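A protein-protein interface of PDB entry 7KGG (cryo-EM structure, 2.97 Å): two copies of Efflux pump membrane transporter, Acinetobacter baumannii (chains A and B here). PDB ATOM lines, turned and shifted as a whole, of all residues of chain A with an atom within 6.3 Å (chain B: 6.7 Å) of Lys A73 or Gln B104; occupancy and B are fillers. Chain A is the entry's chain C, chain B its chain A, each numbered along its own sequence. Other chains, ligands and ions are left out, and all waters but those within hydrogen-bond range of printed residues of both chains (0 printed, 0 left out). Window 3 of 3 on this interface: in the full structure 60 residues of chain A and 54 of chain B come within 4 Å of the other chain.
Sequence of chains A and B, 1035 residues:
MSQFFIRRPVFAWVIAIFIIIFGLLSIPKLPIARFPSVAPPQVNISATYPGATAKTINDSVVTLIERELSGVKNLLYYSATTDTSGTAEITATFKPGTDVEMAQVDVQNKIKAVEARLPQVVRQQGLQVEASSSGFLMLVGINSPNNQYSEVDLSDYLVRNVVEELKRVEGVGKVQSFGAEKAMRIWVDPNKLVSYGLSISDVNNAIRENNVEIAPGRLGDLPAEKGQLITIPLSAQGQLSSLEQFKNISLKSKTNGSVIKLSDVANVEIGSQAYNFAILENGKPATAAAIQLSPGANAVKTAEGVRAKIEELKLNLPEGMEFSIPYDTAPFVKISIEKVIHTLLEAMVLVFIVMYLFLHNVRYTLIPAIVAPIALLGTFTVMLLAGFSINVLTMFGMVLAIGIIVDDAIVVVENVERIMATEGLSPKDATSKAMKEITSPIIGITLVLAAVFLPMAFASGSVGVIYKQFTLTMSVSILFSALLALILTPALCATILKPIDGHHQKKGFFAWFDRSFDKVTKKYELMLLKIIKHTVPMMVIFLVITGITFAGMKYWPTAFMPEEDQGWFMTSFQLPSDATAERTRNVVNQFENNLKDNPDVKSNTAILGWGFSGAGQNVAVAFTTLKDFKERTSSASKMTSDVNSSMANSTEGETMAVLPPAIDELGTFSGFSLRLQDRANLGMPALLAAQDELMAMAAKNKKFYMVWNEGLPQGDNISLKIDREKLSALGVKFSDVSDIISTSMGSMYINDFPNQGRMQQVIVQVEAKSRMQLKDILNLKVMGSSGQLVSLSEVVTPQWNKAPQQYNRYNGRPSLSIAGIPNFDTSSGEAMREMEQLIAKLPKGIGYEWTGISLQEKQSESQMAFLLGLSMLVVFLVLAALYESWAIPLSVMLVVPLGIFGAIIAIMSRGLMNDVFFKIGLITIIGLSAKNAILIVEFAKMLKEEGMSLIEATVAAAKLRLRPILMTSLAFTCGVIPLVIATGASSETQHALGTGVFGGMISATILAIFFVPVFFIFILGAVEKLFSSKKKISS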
ATOM      1  N   GLY A  71     -22.136 -15.757   8.915  1.00  0.00           N
ATOM      2  CA  GLY A  71     -21.419 -15.163  10.022  1.00  0.00           C
ATOM      3  C   GLY A  71     -20.158 -15.870  10.468  1.00  0.00           C
ATOM      4  O   GLY A  71     -19.505 -15.400  11.405  1.00  0.00           O
ATOM      5  N   VAL A  72     -19.784 -16.984   9.835  1.00  0.00           N
ATOM      6  CA  VAL A  72     -18.593 -17.708  10.264  1.00  0.00           C
ATOM      7  C   VAL A  72     -17.350 -16.882   9.957  1.00  0.00           C
ATOM      8  O   VAL A  72     -17.343 -16.043   9.046  1.00  0.00           O
ATOM      9  CB  VAL A  72     -18.518 -19.089   9.591  1.00  0.00           C
ATOM     10  CG1 VAL A  72     -19.714 -19.945   9.985  1.00  0.00           C
ATOM     11  CG2 VAL A  72     -18.419 -18.951   8.079  1.00  0.00           C
ATOM     12  N   LYS A  73     -16.290 -17.117  10.725  1.00  0.00           N
ATOM     13  CA  LYS A  73     -15.051 -16.370  10.562  1.00  0.00           C
ATOM     14  C   LYS A  73     -14.218 -16.943   9.421  1.00  0.00           C
ATOM     15  O   LYS A  73     -14.348 -18.113   9.051  1.00  0.00           O
ATOM     16  CB  LYS A  73     -14.225 -16.391  11.852  1.00  0.00           C
ATOM     17  CG  LYS A  73     -15.024 -16.157  13.139  1.00  0.00           C
ATOM     18  CD  LYS A  73     -14.307 -16.665  14.398  1.00  0.00           C
ATOM     19  CE  LYS A  73     -13.878 -18.126  14.301  1.00  0.00           C
ATOM     20  NZ  LYS A  73     -13.475 -18.679  15.623  1.00  0.00           N
ATOM     21  N   ASN A  74     -13.350 -16.097   8.865  1.00  0.00           N
ATOM     22  CA  ASN A  74     -12.401 -16.478   7.823  1.00  0.00           C
ATOM     23  C   ASN A  74     -13.084 -17.028   6.578  1.00  0.00           C
ATOM     24  O   ASN A  74     -12.527 -17.896   5.899  1.00  0.00           O
ATOM     25  CB  ASN A  74     -11.391 -17.503   8.350  1.00  0.00           C
ATOM     26  CG  ASN A  74     -10.627 -17.002   9.559  1.00  0.00           C
ATOM     27  OD1 ASN A  74     -11.139 -17.010  10.678  1.00  0.00           O
ATOM     28  ND2 ASN A  74      -9.393 -16.564   9.340  1.00  0.00           N
ATOM     29  N   LEU A  75     -14.277 -16.539   6.257  1.00  0.00           N
ATOM     30  CA  LEU A  75     -15.030 -17.057   5.125  1.00  0.00           C
ATOM     31  C   LEU A  75     -14.707 -16.281   3.855  1.00  0.00           C
ATOM     32  O   LEU A  75     -14.718 -15.047   3.841  1.00  0.00           O
ATOM     33  CB  LEU A  75     -16.529 -16.986   5.411  1.00  0.00           C
ATOM     34  CG  LEU A  75     -17.447 -17.648   4.382  1.00  0.00           C
ATOM     35  CD1 LEU A  75     -17.480 -19.153   4.576  1.00  0.00           C
ATOM     36  CD2 LEU A  75     -18.846 -17.066   4.478  1.00  0.00           C
ATOM     37  N   PHE A  94     -13.324 -21.067   2.561  1.00  0.00           N
ATOM     38  CA  PHE A  94     -12.682 -20.141   3.482  1.00  0.00           C
ATOM     39  C   PHE A  94     -11.395 -19.594   2.878  1.00  0.00           C
ATOM     40  O   PHE A  94     -10.851 -20.138   1.913  1.00  0.00           O
ATOM     41  CB  PHE A  94     -12.392 -20.828   4.821  1.00  0.00           C
ATOM     42  CG  PHE A  94     -13.629 -21.250   5.558  1.00  0.00           C
ATOM     43  CD1 PHE A  94     -14.266 -22.439   5.249  1.00  0.00           C
ATOM     44  CD2 PHE A  94     -14.161 -20.453   6.557  1.00  0.00           C
ATOM     45  CE1 PHE A  94     -15.408 -22.827   5.920  1.00  0.00           C
ATOM     46  CE2 PHE A  94     -15.303 -20.836   7.235  1.00  0.00           C
ATOM     47  CZ  PHE A  94     -15.927 -22.024   6.915  1.00  0.00           C
ATOM     48  N   LYS A  95     -10.915 -18.500   3.464  1.00  0.00           N
ATOM     49  CA  LYS A  95      -9.741 -17.827   2.936  1.00  0.00           C
ATOM     50  C   LYS A  95      -8.514 -18.733   3.050  1.00  0.00           C
ATOM     51  O   LYS A  95      -8.470 -19.627   3.901  1.00  0.00           O
ATOM     52  CB  LYS A  95      -9.493 -16.517   3.682  1.00  0.00           C
ATOM     53  CG  LYS A  95     -10.575 -15.468   3.472  1.00  0.00           C
ATOM     54  CD  LYS A  95     -10.260 -14.187   4.228  1.00  0.00           C
ATOM     55  CE  LYS A  95     -11.293 -13.106   3.948  1.00  0.00           C
ATOM     56  NZ  LYS A  95     -12.635 -13.453   4.490  1.00  0.00           N
ATOM     57  N   THR A  98      -6.561 -21.113   6.340  1.00  0.00           N
ATOM     58  CA  THR A  98      -7.498 -21.330   7.434  1.00  0.00           C
ATOM     59  C   THR A  98      -7.550 -22.813   7.775  1.00  0.00           C
ATOM     60  O   THR A  98      -7.707 -23.654   6.885  1.00  0.00           O
ATOM     61  CB  THR A  98      -8.895 -20.828   7.064  1.00  0.00           C
ATOM     62  OG1 THR A  98      -8.804 -19.504   6.523  1.00  0.00           O
ATOM     63  CG2 THR A  98      -9.801 -20.812   8.286  1.00  0.00           C
ATOM     64  N   MET A 102     -10.986 -25.892  12.497  1.00  0.00           N
ATOM     65  CA  MET A 102     -11.484 -24.704  13.174  1.00  0.00           C
ATOM     66  C   MET A 102     -12.618 -24.098  12.385  1.00  0.00           C
ATOM     67  O   MET A 102     -13.372 -23.404  13.032  1.00  0.00           O
ATOM     68  CB  MET A 102     -10.308 -23.777  13.415  1.00  0.00           C
ATOM     69  CG  MET A 102      -9.342 -24.302  14.468  1.00  0.00           C
ATOM     70  SD  MET A 102      -8.402 -22.957  15.206  1.00  0.00           S
ATOM     71  CE  MET A 102      -6.935 -23.806  15.779  1.00  0.00           C
ATOM     72  N   ALA A 103     -12.682 -24.220  11.077  1.00  0.00           N
ATOM     73  CA  ALA A 103     -13.821 -23.846  10.250  1.00  0.00           C
ATOM     74  C   ALA A 103     -14.989 -24.797  10.468  1.00  0.00           C
ATOM     75  O   ALA A 103     -16.139 -24.363  10.581  1.00  0.00           O
ATOM     76  CB  ALA A 103     -13.412 -23.828   8.779  1.00  0.00           C
ATOM     77  N   ASP A 106     -16.605 -24.183  13.939  1.00  0.00           N
ATOM     78  CA  ASP A 106     -17.374 -22.943  13.912  1.00  0.00           C
ATOM     79  C   ASP A 106     -18.665 -23.118  13.122  1.00  0.00           C
ATOM     80  O   ASP A 106     -19.731 -22.647  13.541  1.00  0.00           O
ATOM     81  CB  ASP A 106     -16.531 -21.816  13.314  1.00  0.00           C
ATOM     82  CG  ASP A 106     -17.201 -20.460  13.431  1.00  0.00           C
ATOM     83  OD1 ASP A 106     -18.318 -20.390  13.987  1.00  0.00           O
ATOM     84  OD2 ASP A 106     -16.616 -19.463  12.961  1.00  0.00           O
ATOM     85  N   ASN A 109     -21.154 -25.112  15.177  1.00  0.00           N
ATOM     86  CA  ASN A 109     -21.698 -24.314  16.270  1.00  0.00           C
ATOM     87  C   ASN A 109     -22.729 -23.315  15.760  1.00  0.00           C
ATOM     88  O   ASN A 109     -23.762 -23.098  16.405  1.00  0.00           O
ATOM     89  CB  ASN A 109     -20.567 -23.596  17.004  1.00  0.00           C
ATOM     90  CG  ASN A 109     -19.923 -24.460  18.072  1.00  0.00           C
ATOM     91  OD1 ASN A 109     -20.406 -25.549  18.384  1.00  0.00           O
ATOM     92  ND2 ASN A 109     -18.823 -23.978  18.636  1.00  0.00           N
ATOM     93  N   VAL B  43     -13.936 -13.069  25.072  1.00  0.00           N
ATOM     94  CA  VAL B  43     -14.772 -14.055  24.395  1.00  0.00           C
ATOM     95  C   VAL B  43     -16.105 -14.124  25.126  1.00  0.00           C
ATOM     96  O   VAL B  43     -16.136 -14.250  26.357  1.00  0.00           O
ATOM     97  CB  VAL B  43     -14.100 -15.439  24.344  1.00  0.00           C
ATOM     98  CG1 VAL B  43     -14.902 -16.386  23.465  1.00  0.00           C
ATOM     99  CG2 VAL B  43     -12.673 -15.320  23.827  1.00  0.00           C
ATOM    100  N   ASN B  44     -17.201 -14.044  24.375  1.00  0.00           N
ATOM    101  CA  ASN B  44     -18.540 -13.937  24.932  1.00  0.00           C
ATOM    102  C   ASN B  44     -19.346 -15.189  24.612  1.00  0.00           C
ATOM    103  O   ASN B  44     -19.399 -15.627  23.456  1.00  0.00           O
ATOM    104  CB  ASN B  44     -19.259 -12.699  24.390  1.00  0.00           C
ATOM    105  CG  ASN B  44     -18.352 -11.488  24.311  1.00  0.00           C
ATOM    106  OD1 ASN B  44     -18.082 -10.833  25.318  1.00  0.00           O
ATOM    107  ND2 ASN B  44     -17.877 -11.182  23.109  1.00  0.00           N
ATOM    108  N   PHE B  94      -8.881 -12.452  28.765  1.00  0.00           N
ATOM    109  CA  PHE B  94      -7.596 -13.126  28.867  1.00  0.00           C
ATOM    110  C   PHE B  94      -6.473 -12.102  28.944  1.00  0.00           C
ATOM    111  O   PHE B  94      -6.677 -10.905  28.726  1.00  0.00           O
ATOM    112  CB  PHE B  94      -7.369 -14.059  27.672  1.00  0.00           C
ATOM    113  CG  PHE B  94      -8.469 -15.057  27.469  1.00  0.00           C
ATOM    114  CD1 PHE B  94      -9.657 -14.688  26.862  1.00  0.00           C
ATOM    115  CD2 PHE B  94      -8.317 -16.366  27.888  1.00  0.00           C
ATOM    116  CE1 PHE B  94     -10.671 -15.604  26.677  1.00  0.00           C
ATOM    117  CE2 PHE B  94      -9.328 -17.285  27.706  1.00  0.00           C
ATOM    118  CZ  PHE B  94     -10.506 -16.904  27.101  1.00  0.00           C
ATOM    119  N   ASP B  99      -3.849 -15.396  21.894  1.00  0.00           N
ATOM    120  CA  ASP B  99      -4.513 -15.628  20.617  1.00  0.00           C
ATOM    121  C   ASP B  99      -6.001 -15.849  20.856  1.00  0.00           C
ATOM    122  O   ASP B  99      -6.387 -16.694  21.670  1.00  0.00           O
ATOM    123  CB  ASP B  99      -3.894 -16.825  19.902  1.00  0.00           C
ATOM    124  CG  ASP B  99      -4.611 -17.165  18.610  1.00  0.00           C
ATOM    125  OD1 ASP B  99      -5.099 -16.234  17.937  1.00  0.00           O
ATOM    126  OD2 ASP B  99      -4.685 -18.363  18.268  1.00  0.00           O
ATOM    127  N   VAL B 100      -6.836 -15.089  20.145  1.00  0.00           N
ATOM    128  CA  VAL B 100      -8.276 -15.147  20.380  1.00  0.00           C
ATOM    129  C   VAL B 100      -8.847 -16.483  19.924  1.00  0.00           C
ATOM    130  O   VAL B 100      -9.736 -17.046  20.573  1.00  0.00           O
ATOM    131  CB  VAL B 100      -8.978 -13.965  19.686  1.00  0.00           C
ATOM    132  CG1 VAL B 100      -8.482 -12.650  20.258  1.00  0.00           C
ATOM    133  CG2 VAL B 100      -8.767 -14.014  18.176  1.00  0.00           C
ATOM    134  N   GLU B 101      -8.358 -17.009  18.799  1.00  0.00           N
ATOM    135  CA  GLU B 101      -8.938 -18.230  18.247  1.00  0.00           C
ATOM    136  C   GLU B 101      -8.737 -19.418  19.181  1.00  0.00           C
ATOM    137  O   GLU B 101      -9.688 -20.153  19.473  1.00  0.00           O
ATOM    138  CB  GLU B 101      -8.330 -18.517  16.874  1.00  0.00           C
ATOM    139  CG  GLU B 101      -8.650 -17.456  15.827  1.00  0.00           C
ATOM    140  CD  GLU B 101      -8.793 -18.021  14.424  1.00  0.00           C
ATOM    141  OE1 GLU B 101      -8.958 -19.251  14.281  1.00  0.00           O
ATOM    142  OE2 GLU B 101      -8.740 -17.229  13.459  1.00  0.00           O
ATOM    143  N   MET B 102      -7.538 -19.496  19.706  1.00  0.00           N
ATOM    144  CA  MET B 102      -7.208 -20.674  20.504  1.00  0.00           C
ATOM    145  C   MET B 102      -7.820 -20.535  21.869  1.00  0.00           C
ATOM    146  O   MET B 102      -7.944 -21.564  22.464  1.00  0.00           O
ATOM    147  CB  MET B 102      -5.702 -20.893  20.590  1.00  0.00           C
ATOM    148  CG  MET B 102      -5.094 -21.551  19.370  1.00  0.00           C
ATOM    149  SD  MET B 102      -6.030 -22.937  18.672  1.00  0.00           S
ATOM    150  CE  MET B 102      -6.273 -24.012  20.084  1.00  0.00           C
ATOM    151  N   ALA B 103      -8.019 -19.346  22.386  1.00  0.00           N
ATOM    152  CA  ALA B 103      -8.748 -19.103  23.626  1.00  0.00           C
ATOM    153  C   ALA B 103     -10.222 -19.450  23.469  1.00  0.00           C
ATOM    154  O   ALA B 103     -10.820 -20.082  24.348  1.00  0.00           O
ATOM    155  CB  ALA B 103      -8.581 -17.644  24.049  1.00  0.00           C
ATOM    156  N   GLN B 104     -10.823 -19.053  22.345  1.00  0.00           N
ATOM    157  CA  GLN B 104     -12.212 -19.410  22.076  1.00  0.00           C
ATOM    158  C   GLN B 104     -12.377 -20.920  21.972  1.00  0.00           C
ATOM    159  O   GLN B 104     -13.366 -21.481  22.454  1.00  0.00           O
ATOM    160  CB  GLN B 104     -12.680 -18.728  20.790  1.00  0.00           C
ATOM    161  CG  GLN B 104     -14.135 -18.983  20.443  1.00  0.00           C
ATOM    162  CD  GLN B 104     -14.586 -18.202  19.224  1.00  0.00           C
ATOM    163  OE1 GLN B 104     -13.877 -17.320  18.739  1.00  0.00           O
ATOM    164  NE2 GLN B 104     -15.772 -18.525  18.719  1.00  0.00           N
ATOM    165  N   VAL B 105     -11.418 -21.592  21.330  1.00  0.00           N
ATOM    166  CA  VAL B 105     -11.493 -23.044  21.195  1.00  0.00           C
ATOM    167  C   VAL B 105     -11.449 -23.710  22.564  1.00  0.00           C
ATOM    168  O   VAL B 105     -12.214 -24.640  22.843  1.00  0.00           O
ATOM    169  CB  VAL B 105     -10.361 -23.547  20.283  1.00  0.00           C
ATOM    170  CG1 VAL B 105     -10.293 -25.068  20.303  1.00  0.00           C
ATOM    171  CG2 VAL B 105     -10.560 -23.036  18.869  1.00  0.00           C
ATOM    172  N   ASP B 106     -10.545 -23.253  23.433  1.00  0.00           N
ATOM    173  CA  ASP B 106     -10.466 -23.810  24.780  1.00  0.00           C
ATOM    174  C   ASP B 106     -11.752 -23.553  25.555  1.00  0.00           C
ATOM    175  O   ASP B 106     -12.239 -24.431  26.279  1.00  0.00           O
ATOM    176  CB  ASP B 106      -9.267 -23.217  25.522  1.00  0.00           C
ATOM    177  CG  ASP B 106      -8.890 -24.016  26.755  1.00  0.00           C
ATOM    178  OD1 ASP B 106      -9.699 -24.862  27.191  1.00  0.00           O
ATOM    179  OD2 ASP B 106      -7.784 -23.795  27.292  1.00  0.00           O
ATOM    180  N   VAL B 107     -12.312 -22.350  25.421  1.00  0.00           N
ATOM    181  CA  VAL B 107     -13.561 -22.037  26.106  1.00  0.00           C
ATOM    182  C   VAL B 107     -14.669 -22.973  25.641  1.00  0.00           C
ATOM    183  O   VAL B 107     -15.430 -23.509  26.454  1.00  0.00           O
ATOM    184  CB  VAL B 107     -13.933 -20.560  25.883  1.00  0.00           C
ATOM    185  CG1 VAL B 107     -15.420 -20.333  26.122  1.00  0.00           C
ATOM    186  CG2 VAL B 107     -13.099 -19.662  26.785  1.00  0.00           C
ATOM    187  N   GLN B 108     -14.776 -23.188  24.329  1.00  0.00           N
ATOM    188  CA  GLN B 108     -15.798 -24.089  23.806  1.00  0.00           C
ATOM    189  C   GLN B 108     -15.579 -25.515  24.299  1.00  0.00           C
ATOM    190  O   GLN B 108     -16.537 -26.206  24.670  1.00  0.00           O
ATOM    191  CB  GLN B 108     -15.797 -24.044  22.279  1.00  0.00           C
ATOM    192  CG  GLN B 108     -16.324 -22.740  21.703  1.00  0.00           C
ATOM    193  CD  GLN B 108     -15.868 -22.507  20.276  1.00  0.00           C
ATOM    194  OE1 GLN B 108     -14.726 -22.801  19.921  1.00  0.00           O
ATOM    195  NE2 GLN B 108     -16.758 -21.969  19.451  1.00  0.00           N
ATOM    196  N   ASN B 109     -14.325 -25.972  24.305  1.00  0.00           N
ATOM    197  CA  ASN B 109     -14.027 -27.324  24.763  1.00  0.00           C
ATOM    198  C   ASN B 109     -14.438 -27.507  26.218  1.00  0.00           C
ATOM    199  O   ASN B 109     -15.011 -28.536  26.590  1.00  0.00           O
ATOM    200  CB  ASN B 109     -12.538 -27.620  24.584  1.00  0.00           C
ATOM    201  CG  ASN B 109     -12.175 -27.948  23.149  1.00  0.00           C
ATOM    202  OD1 ASN B 109     -13.046 -28.210  22.319  1.00  0.00           O
ATOM    203  ND2 ASN B 109     -10.883 -27.932  22.848  1.00  0.00           N
ATOM    204  N   ILE B 111     -16.710 -25.744  27.754  1.00  0.00           N
ATOM    205  CA  ILE B 111     -18.163 -25.644  27.801  1.00  0.00           C
ATOM    206  C   ILE B 111     -18.827 -26.956  27.415  1.00  0.00           C
ATOM    207  O   ILE B 111     -19.928 -27.249  27.893  1.00  0.00           O
ATOM    208  CB  ILE B 111     -18.654 -24.507  26.884  1.00  0.00           C
ATOM    209  CG1 ILE B 111     -18.288 -23.148  27.481  1.00  0.00           C
ATOM    210  CG2 ILE B 111     -20.160 -24.602  26.671  1.00  0.00           C
ATOM    211  CD1 ILE B 111     -18.367 -22.009  26.487  1.00  0.00           C
ATOM    212  N   VAL B 129     -20.853 -19.043  21.107  1.00  0.00           N
ATOM    213  CA  VAL B 129     -19.580 -18.534  21.605  1.00  0.00           C
ATOM    214  C   VAL B 129     -18.927 -17.737  20.484  1.00  0.00           C
ATOM    215  O   VAL B 129     -18.770 -18.244  19.366  1.00  0.00           O
ATOM    216  CB  VAL B 129     -18.670 -19.676  22.081  1.00  0.00           C
ATOM    217  CG1 VAL B 129     -17.266 -19.160  22.362  1.00  0.00           C
ATOM    218  CG2 VAL B 129     -19.265 -20.351  23.307  1.00  0.00           C
ATOM    219  N   GLU B 130     -18.545 -16.493  20.771  1.00  0.00           N
ATOM    220  CA  GLU B 130     -17.963 -15.640  19.743  1.00  0.00           C
ATOM    221  C   GLU B 130     -16.978 -14.665  20.370  1.00  0.00           C
ATOM    222  O   GLU B 130     -17.149 -14.249  21.517  1.00  0.00           O
ATOM    223  CB  GLU B 130     -19.051 -14.874  18.979  1.00  0.00           C
ATOM    224  CG  GLU B 130     -19.901 -13.952  19.847  1.00  0.00           C
ATOM    225  CD  GLU B 130     -19.302 -12.565  20.006  1.00  0.00           C
ATOM    226  OE1 GLU B 130     -18.452 -12.179  19.175  1.00  0.00           O
ATOM    227  OE2 GLU B 130     -19.681 -11.861  20.964  1.00  0.00           O
ATOM    228  N   ALA B 131     -15.959 -14.288  19.602  1.00  0.00           N
ATOM    229  CA  ALA B 131     -14.953 -13.341  20.063  1.00  0.00           C
ATOM    230  C   ALA B 131     -15.268 -11.952  19.522  1.00  0.00           C
ATOM    231  O   ALA B 131     -15.395 -11.764  18.309  1.00  0.00           O
ATOM    232  CB  ALA B 131     -13.556 -13.778  19.621  1.00  0.00           C
ATOM    233  N   PRO B 295     -12.472  -9.091  16.103  1.00  0.00           N
ATOM    234  CA  PRO B 295     -11.222  -9.069  16.872  1.00  0.00           C
ATOM    235  C   PRO B 295     -10.011  -9.084  15.951  1.00  0.00           C
ATOM    236  O   PRO B 295      -9.994  -9.767  14.926  1.00  0.00           O
ATOM    237  CB  PRO B 295     -11.308 -10.340  17.723  1.00  0.00           C
ATOM    238  CG  PRO B 295     -12.208 -11.244  16.953  1.00  0.00           C
ATOM    239  CD  PRO B 295     -13.223 -10.341  16.314  1.00  0.00           C
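Met A102 touches its own counterpart, Met B102. 5 positions are printed for both chains. Of the 5 pairs that touch across the chains among the printed residues, 1 has its exchanged pair printed and touching as well.
The side-chain amide oxygen (OE1) of Gln B104 sits at hydrogen-bond distance from the side-chain amino group (NZ) of Lys A73, at 3.4 Å. NE2 of Gln B108 sits close to ND2 of Asn A109 (3.0 Å).
Gln B104 touches just one residue of chain A: Lys A73. Of the printed residues of chain A, Gln B108 touches Asn A109 (3.0 Å). Of the printed residues of chain A, Met B102 touches Met A102 (3.2 Å). Val B105 touches none of the printed residues of chain A. The nearest residue of chain B that does not touch Lys A73 is Glu B101 (4.7 Å). The nearest residue of chain A that does not touch Gln B104 is Asp A106 (5.7 Å).
N of Glu B101 sits close to OD1 of Asp B99. OD2 of Asp B99 lies within hydrogen-bond range of N of Met B102, 3.4 Å away. The side-chain amide oxygen (OE1) of Gln B108 sits close to the backbone carbonyl oxygen (O) of Gln B104. The side-chain amide nitrogen of Gln B104 is in hydrogen-bond range of the backbone carbonyl oxygen of Val B129 (3.1 Å). The backbone NH of Lys A73 lies within hydrogen-bond range of the side-chain carboxylate of Asp A106, at 3.3 Å. O of Asn A74 is in hydrogen-bond range of N of Lys A95.
Among the printed residues, merely in contact across the chains: Met A102 with Met B102, Asn A74 with Glu B101 and Met A102 with Glu B101.
Hydrophobic or aromatic side chains of chain A that line the printed part of chain B: Met A102. Of the 19 printed residues of chain B, 4 touch a printed residue of chain A. Printed residues of chain B that touch a printed residue of chain A: Glu B101, Met B102, Gln B104 and Gln B108. Among the printed residues, 5 pairs touch across the chains. Among the printed residues, no Asp or Glu carboxylate lies within 4 Å of a Lys or Arg side-chain nitrogen of the other chain.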
